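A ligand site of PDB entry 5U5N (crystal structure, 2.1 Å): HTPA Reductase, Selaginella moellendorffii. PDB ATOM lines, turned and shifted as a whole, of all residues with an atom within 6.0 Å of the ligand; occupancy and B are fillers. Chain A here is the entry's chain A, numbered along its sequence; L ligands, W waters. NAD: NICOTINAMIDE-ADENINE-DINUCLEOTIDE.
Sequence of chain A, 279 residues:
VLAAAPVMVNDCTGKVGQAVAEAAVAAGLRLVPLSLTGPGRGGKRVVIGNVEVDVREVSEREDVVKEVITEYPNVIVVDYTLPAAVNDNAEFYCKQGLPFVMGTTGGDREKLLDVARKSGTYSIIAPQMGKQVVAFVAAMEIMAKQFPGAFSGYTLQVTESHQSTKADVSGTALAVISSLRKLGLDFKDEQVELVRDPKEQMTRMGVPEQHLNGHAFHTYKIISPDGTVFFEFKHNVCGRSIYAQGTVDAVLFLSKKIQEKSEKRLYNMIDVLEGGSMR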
ATOM      1  N   ASN A  10      14.888  11.022  23.950  1.00  0.00           N
ATOM      2  CA  ASN A  10      14.998   9.925  22.993  1.00  0.00           C
ATOM      3  C   ASN A  10      16.117  10.265  22.031  1.00  0.00           C
ATOM      4  O   ASN A  10      15.966  11.217  21.266  1.00  0.00           O
ATOM      5  CB  ASN A  10      13.668   9.756  22.249  1.00  0.00           C
ATOM      6  CG  ASN A  10      12.515   9.599  23.213  1.00  0.00           C
ATOM      7  OD1 ASN A  10      12.679   9.047  24.295  1.00  0.00           O
ATOM      8  ND2 ASN A  10      11.338  10.028  22.823  1.00  0.00           N
ATOM      9  N   ASP A  11      17.258   9.582  22.046  1.00  0.00           N
ATOM     10  CA  ASP A  11      17.581   8.329  22.715  1.00  0.00           C
ATOM     11  C   ASP A  11      18.659   8.651  23.729  1.00  0.00           C
ATOM     12  O   ASP A  11      19.720   9.092  23.338  1.00  0.00           O
ATOM     13  CB  ASP A  11      18.123   7.386  21.622  1.00  0.00           C
ATOM     14  CG  ASP A  11      18.595   6.024  22.138  1.00  0.00           C
ATOM     15  OD1 ASP A  11      18.550   5.711  23.353  1.00  0.00           O
ATOM     16  OD2 ASP A  11      19.053   5.222  21.278  1.00  0.00           O
ATOM     17  N   THR A  13      20.674   6.752  25.087  1.00  0.00           N
ATOM     18  CA  THR A  13      21.857   5.917  24.830  1.00  0.00           C
ATOM     19  C   THR A  13      22.680   6.343  23.644  1.00  0.00           C
ATOM     20  O   THR A  13      23.789   5.872  23.503  1.00  0.00           O
ATOM     21  CB  THR A  13      21.458   4.421  24.577  1.00  0.00           C
ATOM     22  OG1 THR A  13      20.714   4.292  23.353  1.00  0.00           O
ATOM     23  CG2 THR A  13      20.634   3.909  25.708  1.00  0.00           C
ATOM     24  N   GLY A  14      22.142   7.176  22.775  1.00  0.00           N
ATOM     25  CA  GLY A  14      22.953   7.812  21.723  1.00  0.00           C
ATOM     26  C   GLY A  14      23.945   8.807  22.303  1.00  0.00           C
ATOM     27  O   GLY A  14      23.846   9.155  23.472  1.00  0.00           O
ATOM     28  N   LYS A  15      24.916   9.254  21.524  1.00  0.00           N
ATOM     29  CA  LYS A  15      26.009  10.068  22.078  1.00  0.00           C
ATOM     30  C   LYS A  15      25.544  11.448  22.525  1.00  0.00           C
ATOM     31  O   LYS A  15      25.841  11.842  23.633  1.00  0.00           O
ATOM     32  CB  LYS A  15      27.162  10.226  21.103  1.00  0.00           C
ATOM     33  CG  LYS A  15      27.648   8.931  20.511  1.00  0.00           C
ATOM     34  CD  LYS A  15      29.134   8.780  20.577  1.00  0.00           C
ATOM     35  CE  LYS A  15      29.550   7.749  19.562  1.00  0.00           C
ATOM     36  NZ  LYS A  15      29.670   8.399  18.216  1.00  0.00           N
ATOM     37  N   VAL A  16      24.795  12.138  21.674  1.00  0.00           N
ATOM     38  CA  VAL A  16      24.280  13.482  21.970  1.00  0.00           C
ATOM     39  C   VAL A  16      23.112  13.410  22.931  1.00  0.00           C
ATOM     40  O   VAL A  16      22.990  14.260  23.823  1.00  0.00           O
ATOM     41  CB  VAL A  16      23.850  14.250  20.682  1.00  0.00           C
ATOM     42  CG1 VAL A  16      23.264  15.627  21.003  1.00  0.00           C
ATOM     43  CG2 VAL A  16      25.049  14.427  19.747  1.00  0.00           C
ATOM     44  N   GLY A  17      22.230  12.434  22.710  1.00  0.00           N
ATOM     45  CA  GLY A  17      21.117  12.139  23.604  1.00  0.00           C
ATOM     46  C   GLY A  17      21.553  11.918  25.048  1.00  0.00           C
ATOM     47  O   GLY A  17      20.995  12.555  25.932  1.00  0.00           O
ATOM     48  N   LEU A  36      13.255   5.994  24.518  1.00  0.00           N
ATOM     49  CA  LEU A  36      12.997   5.151  23.360  1.00  0.00           C
ATOM     50  C   LEU A  36      14.305   5.068  22.595  1.00  0.00           C
ATOM     51  O   LEU A  36      14.977   6.109  22.387  1.00  0.00           O
ATOM     52  CB  LEU A  36      11.878   5.740  22.516  1.00  0.00           C
ATOM     53  CG  LEU A  36      10.507   5.591  23.168  1.00  0.00           C
ATOM     54  CD1 LEU A  36       9.466   6.455  22.520  1.00  0.00           C
ATOM     55  CD2 LEU A  36      10.038   4.131  23.101  1.00  0.00           C
ATOM     56  N   THR A  37      14.698   3.851  22.241  1.00  0.00           N
ATOM     57  CA  THR A  37      15.929   3.627  21.500  1.00  0.00           C
ATOM     58  C   THR A  37      15.524   3.086  20.136  1.00  0.00           C
ATOM     59  O   THR A  37      14.323   2.888  19.876  1.00  0.00           O
ATOM     60  CB  THR A  37      16.948   2.723  22.266  1.00  0.00           C
ATOM     61  OG1 THR A  37      18.190   2.702  21.568  1.00  0.00           O
ATOM     62  CG2 THR A  37      16.430   1.285  22.473  1.00  0.00           C
ATOM     63  N   GLY A  38      16.507   2.921  19.257  1.00  0.00           N
ATOM     64  CA  GLY A  38      16.209   2.732  17.822  1.00  0.00           C
ATOM     65  C   GLY A  38      15.925   1.309  17.449  1.00  0.00           C
ATOM     66  O   GLY A  38      16.135   0.404  18.246  1.00  0.00           O
ATOM     67  N   PRO A  39      15.473   1.097  16.199  1.00  0.00           N
ATOM     68  CA  PRO A  39      15.099  -0.261  15.824  1.00  0.00           C
ATOM     69  C   PRO A  39      16.397  -1.073  15.804  1.00  0.00           C
ATOM     70  O   PRO A  39      17.477  -0.535  15.499  1.00  0.00           O
ATOM     71  CB  PRO A  39      14.496  -0.094  14.433  1.00  0.00           C
ATOM     72  CG  PRO A  39      15.125   1.162  13.869  1.00  0.00           C
ATOM     73  CD  PRO A  39      15.590   1.995  15.029  1.00  0.00           C
ATOM     74  N   ARG A  41      17.956  -1.986  18.556  1.00  0.00           N
ATOM     75  CA  ARG A  41      18.565  -1.897  19.883  1.00  0.00           C
ATOM     76  C   ARG A  41      17.606  -2.517  20.921  1.00  0.00           C
ATOM     77  O   ARG A  41      16.391  -2.393  20.793  1.00  0.00           O
ATOM     78  CB  ARG A  41      18.839  -0.447  20.248  1.00  0.00           C
ATOM     79  CG  ARG A  41      19.745   0.329  19.282  1.00  0.00           C
ATOM     80  CD  ARG A  41      21.208  -0.077  19.323  1.00  0.00           C
ATOM     81  NE  ARG A  41      21.772  -0.156  20.681  1.00  0.00           N
ATOM     82  CZ  ARG A  41      22.956  -0.718  20.982  1.00  0.00           C
ATOM     83  NH1 ARG A  41      23.755  -1.214  20.048  1.00  0.00           N
ATOM     84  NH2 ARG A  41      23.346  -0.776  22.237  1.00  0.00           N
ATOM     85  N   VAL A  58      11.682   0.848  20.363  1.00  0.00           N
ATOM     86  CA  VAL A  58      10.777   1.771  19.673  1.00  0.00           C
ATOM     87  C   VAL A  58       9.463   1.102  19.247  1.00  0.00           C
ATOM     88  O   VAL A  58       8.452   1.772  19.106  1.00  0.00           O
ATOM     89  CB  VAL A  58      11.447   2.482  18.471  1.00  0.00           C
ATOM     90  CG1 VAL A  58      11.695   1.541  17.298  1.00  0.00           C
ATOM     91  CG2 VAL A  58      10.620   3.709  18.089  1.00  0.00           C
ATOM     92  N   ARG A  61       6.513   2.012  21.579  1.00  0.00           N
ATOM     93  CA  ARG A  61       6.402   3.463  21.848  1.00  0.00           C
ATOM     94  C   ARG A  61       5.011   3.980  22.253  1.00  0.00           C
ATOM     95  O   ARG A  61       4.888   4.973  22.933  1.00  0.00           O
ATOM     96  CB  ARG A  61       6.942   4.268  20.687  1.00  0.00           C
ATOM     97  CG  ARG A  61       6.155   4.174  19.396  1.00  0.00           C
ATOM     98  CD  ARG A  61       6.865   4.993  18.350  1.00  0.00           C
ATOM     99  NE  ARG A  61       6.181   4.882  17.064  1.00  0.00           N
ATOM    100  CZ  ARG A  61       6.390   5.675  16.024  1.00  0.00           C
ATOM    101  NH1 ARG A  61       7.282   6.676  16.066  1.00  0.00           N
ATOM    102  NH2 ARG A  61       5.691   5.485  14.915  1.00  0.00           N
ATOM    103  N   ASP A  79      14.356  14.991  21.027  1.00  0.00           N
ATOM    104  CA  ASP A  79      14.701  13.995  20.028  1.00  0.00           C
ATOM    105  C   ASP A  79      16.094  14.229  19.440  1.00  0.00           C
ATOM    106  O   ASP A  79      16.306  15.195  18.703  1.00  0.00           O
ATOM    107  CB  ASP A  79      13.650  13.975  18.922  1.00  0.00           C
ATOM    108  CG  ASP A  79      13.752  12.757  18.027  1.00  0.00           C
ATOM    109  OD1 ASP A  79      14.692  12.697  17.237  1.00  0.00           O
ATOM    110  OD2 ASP A  79      12.872  11.833  18.110  1.00  0.00           O
ATOM    111  N   TYR A  80      17.041  13.367  19.831  1.00  0.00           N
ATOM    112  CA  TYR A  80      18.319  13.161  19.160  1.00  0.00           C
ATOM    113  C   TYR A  80      18.444  11.684  18.809  1.00  0.00           C
ATOM    114  O   TYR A  80      18.996  10.872  19.579  1.00  0.00           O
ATOM    115  CB  TYR A  80      19.497  13.576  20.026  1.00  0.00           C
ATOM    116  CG  TYR A  80      19.711  15.057  20.113  1.00  0.00           C
ATOM    117  CD1 TYR A  80      20.498  15.722  19.165  1.00  0.00           C
ATOM    118  CD2 TYR A  80      19.148  15.801  21.145  1.00  0.00           C
ATOM    119  CE1 TYR A  80      20.727  17.096  19.245  1.00  0.00           C
ATOM    120  CE2 TYR A  80      19.373  17.187  21.246  1.00  0.00           C
ATOM    121  CZ  TYR A  80      20.160  17.831  20.286  1.00  0.00           C
ATOM    122  OH  TYR A  80      20.368  19.204  20.387  1.00  0.00           O
ATOM    123  N   THR A  81      17.933  11.364  17.624  1.00  0.00           N
ATOM    124  CA  THR A  81      17.920  10.041  17.078  1.00  0.00           C
ATOM    125  C   THR A  81      18.781   9.952  15.827  1.00  0.00           C
ATOM    126  O   THR A  81      19.968  10.054  15.921  1.00  0.00           O
ATOM    127  CB  THR A  81      16.452   9.558  16.859  1.00  0.00           C
ATOM    128  OG1 THR A  81      15.748  10.502  16.024  1.00  0.00           O
ATOM    129  CG2 THR A  81      15.745   9.447  18.182  1.00  0.00           C
ATOM    130  N   LEU A  82      18.197   9.732  14.661  1.00  0.00           N
ATOM    131  CA  LEU A  82      18.971   9.426  13.480  1.00  0.00           C
ATOM    132  C   LEU A  82      18.151   9.985  12.343  1.00  0.00           C
ATOM    133  O   LEU A  82      16.910  10.000  12.439  1.00  0.00           O
ATOM    134  CB  LEU A  82      19.152   7.905  13.285  1.00  0.00           C
ATOM    135  CG  LEU A  82      20.136   7.080  14.128  1.00  0.00           C
ATOM    136  CD1 LEU A  82      20.118   5.606  13.773  1.00  0.00           C
ATOM    137  CD2 LEU A  82      21.535   7.638  13.952  1.00  0.00           C
ATOM    138  N   PRO A  83      18.803  10.455  11.266  1.00  0.00           N
ATOM    139  CA  PRO A  83      18.064  11.019  10.146  1.00  0.00           C
ATOM    140  C   PRO A  83      16.891  10.139   9.691  1.00  0.00           C
ATOM    141  O   PRO A  83      15.807  10.650   9.423  1.00  0.00           O
ATOM    142  CB  PRO A  83      19.124  11.160   9.064  1.00  0.00           C
ATOM    143  CG  PRO A  83      20.387  11.415   9.836  1.00  0.00           C
ATOM    144  CD  PRO A  83      20.258  10.618  11.103  1.00  0.00           C
ATOM    145  N   ALA A  85      14.917   8.253  11.407  1.00  0.00           N
ATOM    146  CA  ALA A  85      13.761   8.357  12.298  1.00  0.00           C
ATOM    147  C   ALA A  85      13.099   9.727  12.370  1.00  0.00           C
ATOM    148  O   ALA A  85      12.002   9.839  12.929  1.00  0.00           O
ATOM    149  CB  ALA A  85      14.144   7.940  13.701  1.00  0.00           C
ATOM    150  N   ASP A  88       9.275  10.333  10.975  1.00  0.00           N
ATOM    151  CA  ASP A  88       8.398   9.401  11.659  1.00  0.00           C
ATOM    152  C   ASP A  88       8.230   9.767  13.153  1.00  0.00           C
ATOM    153  O   ASP A  88       7.122   9.888  13.642  1.00  0.00           O
ATOM    154  CB  ASP A  88       8.932   7.986  11.488  1.00  0.00           C
ATOM    155  CG  ASP A  88       7.884   6.967  11.741  1.00  0.00           C
ATOM    156  OD1 ASP A  88       7.153   6.621  10.763  1.00  0.00           O
ATOM    157  OD2 ASP A  88       7.818   6.522  12.918  1.00  0.00           O
ATOM    158  N   ASN A  89       9.343   9.976  13.848  1.00  0.00           N
ATOM    159  CA  ASN A  89       9.290  10.436  15.243  1.00  0.00           C
ATOM    160  C   ASN A  89       8.444  11.715  15.357  1.00  0.00           C
ATOM    161  O   ASN A  89       7.613  11.808  16.225  1.00  0.00           O
ATOM    162  CB  ASN A  89      10.682  10.660  15.848  1.00  0.00           C
ATOM    163  CG  ASN A  89      11.442   9.383  16.089  1.00  0.00           C
ATOM    164  OD1 ASN A  89      10.958   8.297  15.786  1.00  0.00           O
ATOM    165  ND2 ASN A  89      12.641   9.491  16.634  1.00  0.00           N
ATOM    166  N   TYR A  93       5.089  12.318  17.494  1.00  0.00           N
ATOM    167  CA  TYR A  93       4.921  13.328  18.538  1.00  0.00           C
ATOM    168  C   TYR A  93       3.710  14.200  18.287  1.00  0.00           C
ATOM    169  O   TYR A  93       2.937  14.451  19.204  1.00  0.00           O
ATOM    170  CB  TYR A  93       6.173  14.205  18.709  1.00  0.00           C
ATOM    171  CG  TYR A  93       7.441  13.426  18.993  1.00  0.00           C
ATOM    172  CD1 TYR A  93       7.427  12.242  19.760  1.00  0.00           C
ATOM    173  CD2 TYR A  93       8.660  13.864  18.486  1.00  0.00           C
ATOM    174  CE1 TYR A  93       8.581  11.531  20.012  1.00  0.00           C
ATOM    175  CE2 TYR A  93       9.818  13.162  18.729  1.00  0.00           C
ATOM    176  CZ  TYR A  93       9.785  12.009  19.498  1.00  0.00           C
ATOM    177  OH  TYR A  93      10.964  11.330  19.732  1.00  0.00           O
ATOM    178  N   MET A 102      13.427  18.999  18.532  1.00  0.00           N
ATOM    179  CA  MET A 102      14.060  18.141  17.531  1.00  0.00           C
ATOM    180  C   MET A 102      15.439  18.682  17.195  1.00  0.00           C
ATOM    181  O   MET A 102      15.554  19.692  16.504  1.00  0.00           O
ATOM    182  CB  MET A 102      13.157  18.079  16.277  1.00  0.00           C
ATOM    183  CG  MET A 102      13.691  17.324  15.055  1.00  0.00           C
ATOM    184  SD  MET A 102      13.770  15.538  15.388  1.00  0.00           S
ATOM    185  CE  MET A 102      12.029  15.114  15.284  1.00  0.00           C
ATOM    186  N   GLY A 103      16.476  18.015  17.705  1.00  0.00           N
ATOM    187  CA  GLY A 103      17.856  18.364  17.407  1.00  0.00           C
ATOM    188  C   GLY A 103      18.491  17.477  16.323  1.00  0.00           C
ATOM    189  O   GLY A 103      19.589  17.747  15.869  1.00  0.00           O
ATOM    190  N   THR A 104      17.793  16.421  15.920  1.00  0.00           N
ATOM    191  CA  THR A 104      18.317  15.470  14.957  1.00  0.00           C
ATOM    192  C   THR A 104      18.364  16.134  13.584  1.00  0.00           C
ATOM    193  O   THR A 104      17.412  16.777  13.179  1.00  0.00           O
ATOM    194  CB  THR A 104      17.392  14.241  14.891  1.00  0.00           C
ATOM    195  OG1 THR A 104      17.139  13.735  16.202  1.00  0.00           O
ATOM    196  CG2 THR A 104      17.980  13.111  14.005  1.00  0.00           C
ATOM    197  N   THR A 105      19.470  15.968  12.881  1.00  0.00           N
ATOM    198  CA  THR A 105      19.618  16.536  11.549  1.00  0.00           C
ATOM    199  C   THR A 105      19.148  15.512  10.507  1.00  0.00           C
ATOM    200  O   THR A 105      18.848  14.375  10.836  1.00  0.00           O
ATOM    201  CB  THR A 105      21.078  16.914  11.259  1.00  0.00           C
ATOM    202  OG1 THR A 105      21.884  15.735  11.314  1.00  0.00           O
ATOM    203  CG2 THR A 105      21.585  17.922  12.278  1.00  0.00           C
ATOM    204  N   GLY A 106      19.096  15.929   9.252  1.00  0.00           N
ATOM    205  CA  GLY A 106      18.590  15.067   8.192  1.00  0.00           C
ATOM    206  C   GLY A 106      17.091  14.854   8.223  1.00  0.00           C
ATOM    207  O   GLY A 106      16.360  15.469   9.002  1.00  0.00           O
ATOM    208  N   ALA A 126      15.401  22.805  15.397  1.00  0.00           N
ATOM    209  CA  ALA A 126      16.614  23.546  15.119  1.00  0.00           C
ATOM    210  C   ALA A 126      17.754  22.576  14.865  1.00  0.00           C
ATOM    211  O   ALA A 126      18.171  21.832  15.784  1.00  0.00           O
ATOM    212  CB  ALA A 126      16.939  24.456  16.289  1.00  0.00           C
ATOM    213  N   PRO A 127      18.261  22.557  13.621  1.00  0.00           N
ATOM    214  CA  PRO A 127      19.388  21.685  13.303  1.00  0.00           C
ATOM    215  C   PRO A 127      20.771  22.185  13.796  1.00  0.00           C
ATOM    216  O   PRO A 127      21.750  21.443  13.652  1.00  0.00           O
ATOM    217  CB  PRO A 127      19.322  21.622  11.777  1.00  0.00           C
ATOM    218  CG  PRO A 127      18.770  22.940  11.371  1.00  0.00           C
ATOM    219  CD  PRO A 127      17.843  23.356  12.465  1.00  0.00           C
ATOM    220  N   GLN A 128      20.845  23.402  14.333  1.00  0.00           N
ATOM    221  CA  GLN A 128      22.040  23.869  15.082  1.00  0.00           C
ATOM    222  C   GLN A 128      21.574  24.395  16.457  1.00  0.00           C
ATOM    223  O   GLN A 128      20.909  25.411  16.526  1.00  0.00           O
ATOM    224  CB  GLN A 128      22.794  24.933  14.271  1.00  0.00           C
ATOM    225  CG  GLN A 128      23.811  25.798  14.991  1.00  0.00           C
ATOM    226  CD  GLN A 128      25.027  25.068  15.471  1.00  0.00           C
ATOM    227  OE1 GLN A 128      25.066  24.553  16.580  1.00  0.00           O
ATOM    228  NE2 GLN A 128      26.054  25.079  14.652  1.00  0.00           N
ATOM    229  N   MET A 129      21.928  23.664  17.509  1.00  0.00           N
ATOM    230  CA  MET A 129      21.489  23.945  18.877  1.00  0.00           C
ATOM    231  C   MET A 129      22.586  24.565  19.730  1.00  0.00           C
ATOM    232  O   MET A 129      22.336  24.897  20.903  1.00  0.00           O
ATOM    233  CB  MET A 129      20.967  22.664  19.566  1.00  0.00           C
ATOM    234  CG  MET A 129      19.766  22.086  18.861  1.00  0.00           C
ATOM    235  SD  MET A 129      18.244  22.956  19.263  1.00  0.00           S
ATOM    236  CE  MET A 129      17.883  22.168  20.820  1.00  0.00           C
ATOM    237  N   GLY A 130      23.782  24.705  19.173  1.00  0.00           N
ATOM    238  CA  GLY A 130      24.817  25.475  19.847  1.00  0.00           C
ATOM    239  C   GLY A 130      24.449  26.943  19.795  1.00  0.00           C
ATOM    240  O   GLY A 130      24.923  27.668  18.882  1.00  0.00           O
ATOM    241  N   ARG A 240      30.501  18.008  22.687  1.00  0.00           N
ATOM    242  CA  ARG A 240      29.035  18.098  22.556  1.00  0.00           C
ATOM    243  C   ARG A 240      28.347  19.004  23.542  1.00  0.00           C
ATOM    244  O   ARG A 240      27.124  19.175  23.457  1.00  0.00           O
ATOM    245  CB  ARG A 240      28.414  16.699  22.759  1.00  0.00           C
ATOM    246  CG  ARG A 240      28.744  15.781  21.655  1.00  0.00           C
ATOM    247  CD  ARG A 240      28.129  14.404  21.789  1.00  0.00           C
ATOM    248  NE  ARG A 240      28.966  13.529  20.970  1.00  0.00           N
ATOM    249  CZ  ARG A 240      29.961  12.785  21.417  1.00  0.00           C
ATOM    250  NH1 ARG A 240      30.242  12.722  22.726  1.00  0.00           N
ATOM    251  NH2 ARG A 240      30.664  12.077  20.553  1.00  0.00           N
ATOM    252  N   TYR A 243      25.875  21.830  22.511  1.00  0.00           N
ATOM    253  CA  TYR A 243      24.590  21.330  21.984  1.00  0.00           C
ATOM    254  C   TYR A 243      23.704  20.912  23.163  1.00  0.00           C
ATOM    255  O   TYR A 243      22.526  21.255  23.198  1.00  0.00           O
ATOM    256  CB  TYR A 243      24.773  20.214  20.923  1.00  0.00           C
ATOM    257  CG  TYR A 243      25.882  20.560  19.922  1.00  0.00           C
ATOM    258  CD1 TYR A 243      25.729  21.619  19.043  1.00  0.00           C
ATOM    259  CD2 TYR A 243      27.088  19.859  19.893  1.00  0.00           C
ATOM    260  CE1 TYR A 243      26.738  21.975  18.147  1.00  0.00           C
ATOM    261  CE2 TYR A 243      28.107  20.210  19.016  1.00  0.00           C
ATOM    262  CZ  TYR A 243      27.923  21.272  18.148  1.00  0.00           C
ATOM    263  OH  TYR A 243      28.947  21.674  17.305  1.00  0.00           O
HETATM  264  PA  NAD L   1      24.108   8.209  17.766  1.00  0.00           P
HETATM  265  O1A NAD L   1      24.260   7.304  16.559  1.00  0.00           O
HETATM  266  O2A NAD L   1      25.157   8.253  18.853  1.00  0.00           O
HETATM  267  O5B NAD L   1      22.720   7.921  18.490  1.00  0.00           O
HETATM  268  C5B NAD L   1      21.477   8.039  17.831  1.00  0.00           C
HETATM  269  C4B NAD L   1      20.539   7.068  18.545  1.00  0.00           C
HETATM  270  O4B NAD L   1      19.204   7.156  18.048  1.00  0.00           O
HETATM  271  C3B NAD L   1      20.976   5.609  18.404  1.00  0.00           C
HETATM  272  O3B NAD L   1      21.477   5.131  19.669  1.00  0.00           O
HETATM  273  C2B NAD L   1      19.731   4.867  17.881  1.00  0.00           C
HETATM  274  O2B NAD L   1      19.578   3.558  18.464  1.00  0.00           O
HETATM  275  C1B NAD L   1      18.597   5.865  18.187  1.00  0.00           C
HETATM  276  N9A NAD L   1      17.360   5.809  17.366  1.00  0.00           N
HETATM  277  C8A NAD L   1      17.260   5.553  16.050  1.00  0.00           C
HETATM  278  N7A NAD L   1      15.960   5.586  15.648  1.00  0.00           N
HETATM  279  C5A NAD L   1      15.210   5.885  16.728  1.00  0.00           C
HETATM  280  C6A NAD L   1      13.771   6.065  17.003  1.00  0.00           C
HETATM  281  N6A NAD L   1      12.856   5.940  16.016  1.00  0.00           N
HETATM  282  N1A NAD L   1      13.381   6.371  18.260  1.00  0.00           N
HETATM  283  C2A NAD L   1      14.269   6.485  19.268  1.00  0.00           C
HETATM  284  N3A NAD L   1      15.604   6.329  19.089  1.00  0.00           N
HETATM  285  C4A NAD L   1      16.125   6.036  17.858  1.00  0.00           C
HETATM  286  O3  NAD L   1      23.819   9.686  17.180  1.00  0.00           O
HETATM  287  PN  NAD L   1      24.322  11.054  17.901  1.00  0.00           P
HETATM  288  O1N NAD L   1      25.826  11.058  17.777  1.00  0.00           O
HETATM  289  O2N NAD L   1      23.670  11.170  19.266  1.00  0.00           O
HETATM  290  O5D NAD L   1      23.593  12.128  16.935  1.00  0.00           O
HETATM  291  C5D NAD L   1      22.175  12.105  16.805  1.00  0.00           C
HETATM  292  C4D NAD L   1      21.655  13.113  15.796  1.00  0.00           C
HETATM  293  O4D NAD L   1      21.790  14.434  16.337  1.00  0.00           O
HETATM  294  C3D NAD L   1      22.391  13.100  14.454  1.00  0.00           C
HETATM  295  O3D NAD L   1      21.473  13.238  13.354  1.00  0.00           O
HETATM  296  C2D NAD L   1      23.304  14.301  14.528  1.00  0.00           C
HETATM  297  O2D NAD L   1      23.561  14.904  13.254  1.00  0.00           O
HETATM  298  C1D NAD L   1      22.498  15.259  15.392  1.00  0.00           C
HETATM  299  N1N NAD L   1      23.268  16.335  16.045  1.00  0.00           N
HETATM  300  C2N NAD L   1      22.708  17.561  16.014  1.00  0.00           C
HETATM  301  C3N NAD L   1      23.309  18.667  16.595  1.00  0.00           C
HETATM  302  C7N NAD L   1      22.647  20.033  16.527  1.00  0.00           C
HETATM  303  O7N NAD L   1      23.361  21.030  16.585  1.00  0.00           O
HETATM  304  N7N NAD L   1      21.323  20.188  16.375  1.00  0.00           N
HETATM  305  C4N NAD L   1      24.530  18.483  17.230  1.00  0.00           C
HETATM  306  C5N NAD L   1      25.113  17.212  17.267  1.00  0.00           C
HETATM  307  C6N NAD L   1      24.452  16.148  16.661  1.00  0.00           C
HETATM  308  O   HOH W   1      21.358  10.634  20.560  1.00  0.00           O
HETATM  309  O   HOH W   2      25.197   8.482  14.033  1.00  0.00           O
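Water W1 lies within hydrogen-bond range of the backbone carbonyl oxygen of Tyr 80 (2.6 Å), an oxygen (O2N) of the ligand (2.7 Å) and the backbone NH of Gly 17 (2.9 Å).
The backbone NH (N) of Val 58 sits close to the backbone carbonyl oxygen (O) of Thr 37.
OG1 of Thr 104 sits at hydrogen-bond distance from N of Thr 81, 2.9 Å away.
The backbone carbonyl oxygen (O) of Asn 10 is in hydrogen-bond range of the backbone NH (N) of Tyr 80, at 2.8 Å.
The side-chain hydroxyl (OG1) of Thr 81 sits at hydrogen-bond distance from the side-chain amide nitrogen (ND2) of Asn 89 (3.3 Å).
The side-chain amide oxygen (OD1) of Asn 10 is in hydrogen-bond range of the backbone NH (N) of Leu 36, at 3.1 Å.
The backbone carbonyl oxygen (O) of Met 102 is in hydrogen-bond range of the backbone NH (N) of Ala 126.
The backbone NH (N) of Gly 103 sits at hydrogen-bond distance from the backbone carbonyl oxygen (O) of Asp 79 (3.0 Å).
The side-chain amide nitrogen (ND2) of Asn 89 sits at hydrogen-bond distance from the side-chain carboxylate (OD2) of Asp 79 (2.8 Å).
The backbone NH of Thr 105 is in hydrogen-bond range of an oxygen (O3D) of the ligand, at 3.4 Å.
An oxygen (O2B) of the ligand lies within hydrogen-bond range of the backbone NH (N) of Gly 38 (3.2 Å).
The backbone carbonyl oxygen (O) of Gly 103 lies within hydrogen-bond range of a nitrogen (N7N) of the ligand (3.0 Å).
O of Pro 127 is in hydrogen-bond range of N7N of the ligand, at 3.0 Å.
OG1 of Thr 105 sits at hydrogen-bond distance from O2D of the ligand (2.7 Å).
N of Met 129 lies within hydrogen-bond range of O7N of the ligand, at 3.1 Å.
A nitrogen (N6A) of the ligand sits at hydrogen-bond distance from the side-chain amide oxygen (OD1) of Asn 89 (3.0 Å).
N of Lys 15 is in hydrogen-bond range of O2A of the ligand (2.9 Å).
The backbone NH (N) of Val 16 sits at hydrogen-bond distance from an oxygen (O2N) of the ligand, 2.8 Å away.
O3B of the ligand sits at hydrogen-bond distance from OD2 of Asp 11 (2.9 Å).
The backbone carbonyl oxygen (O) of Leu 36 sits close to a nitrogen (N3A) of the ligand, 3.4 Å away.
Residues that only touch the ligand: Thr 81, Gly 14, Ala 85, Arg 41, Tyr 80, Thr 37, Tyr 243, Gln 128, Thr 104, Ala 126, Leu 82, Pro 83, Pro 39, Val 58, Thr 13 and Gly 17.
Hydrophobic or aromatic side chains that line the ligand: Val 16, Pro 39, Val 58, Tyr 80, Leu 82, Pro 83, Ala 85, Met 129 and Tyr 243.
26 residues have an atom within 4 Å of the ligand: Asp 11, Thr 13, Gly 14, Lys 15, Val 16, Gly 17, Leu 36, Thr 37, Gly 38, Pro 39, Arg 41, Val 58, Tyr 80, Thr 81, Leu 82, Pro 83, Ala 85, Asn 89, Gly 103, Thr 104, Thr 105, Ala 126, Pro 127, Gln 128, Met 129 and Tyr 243.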
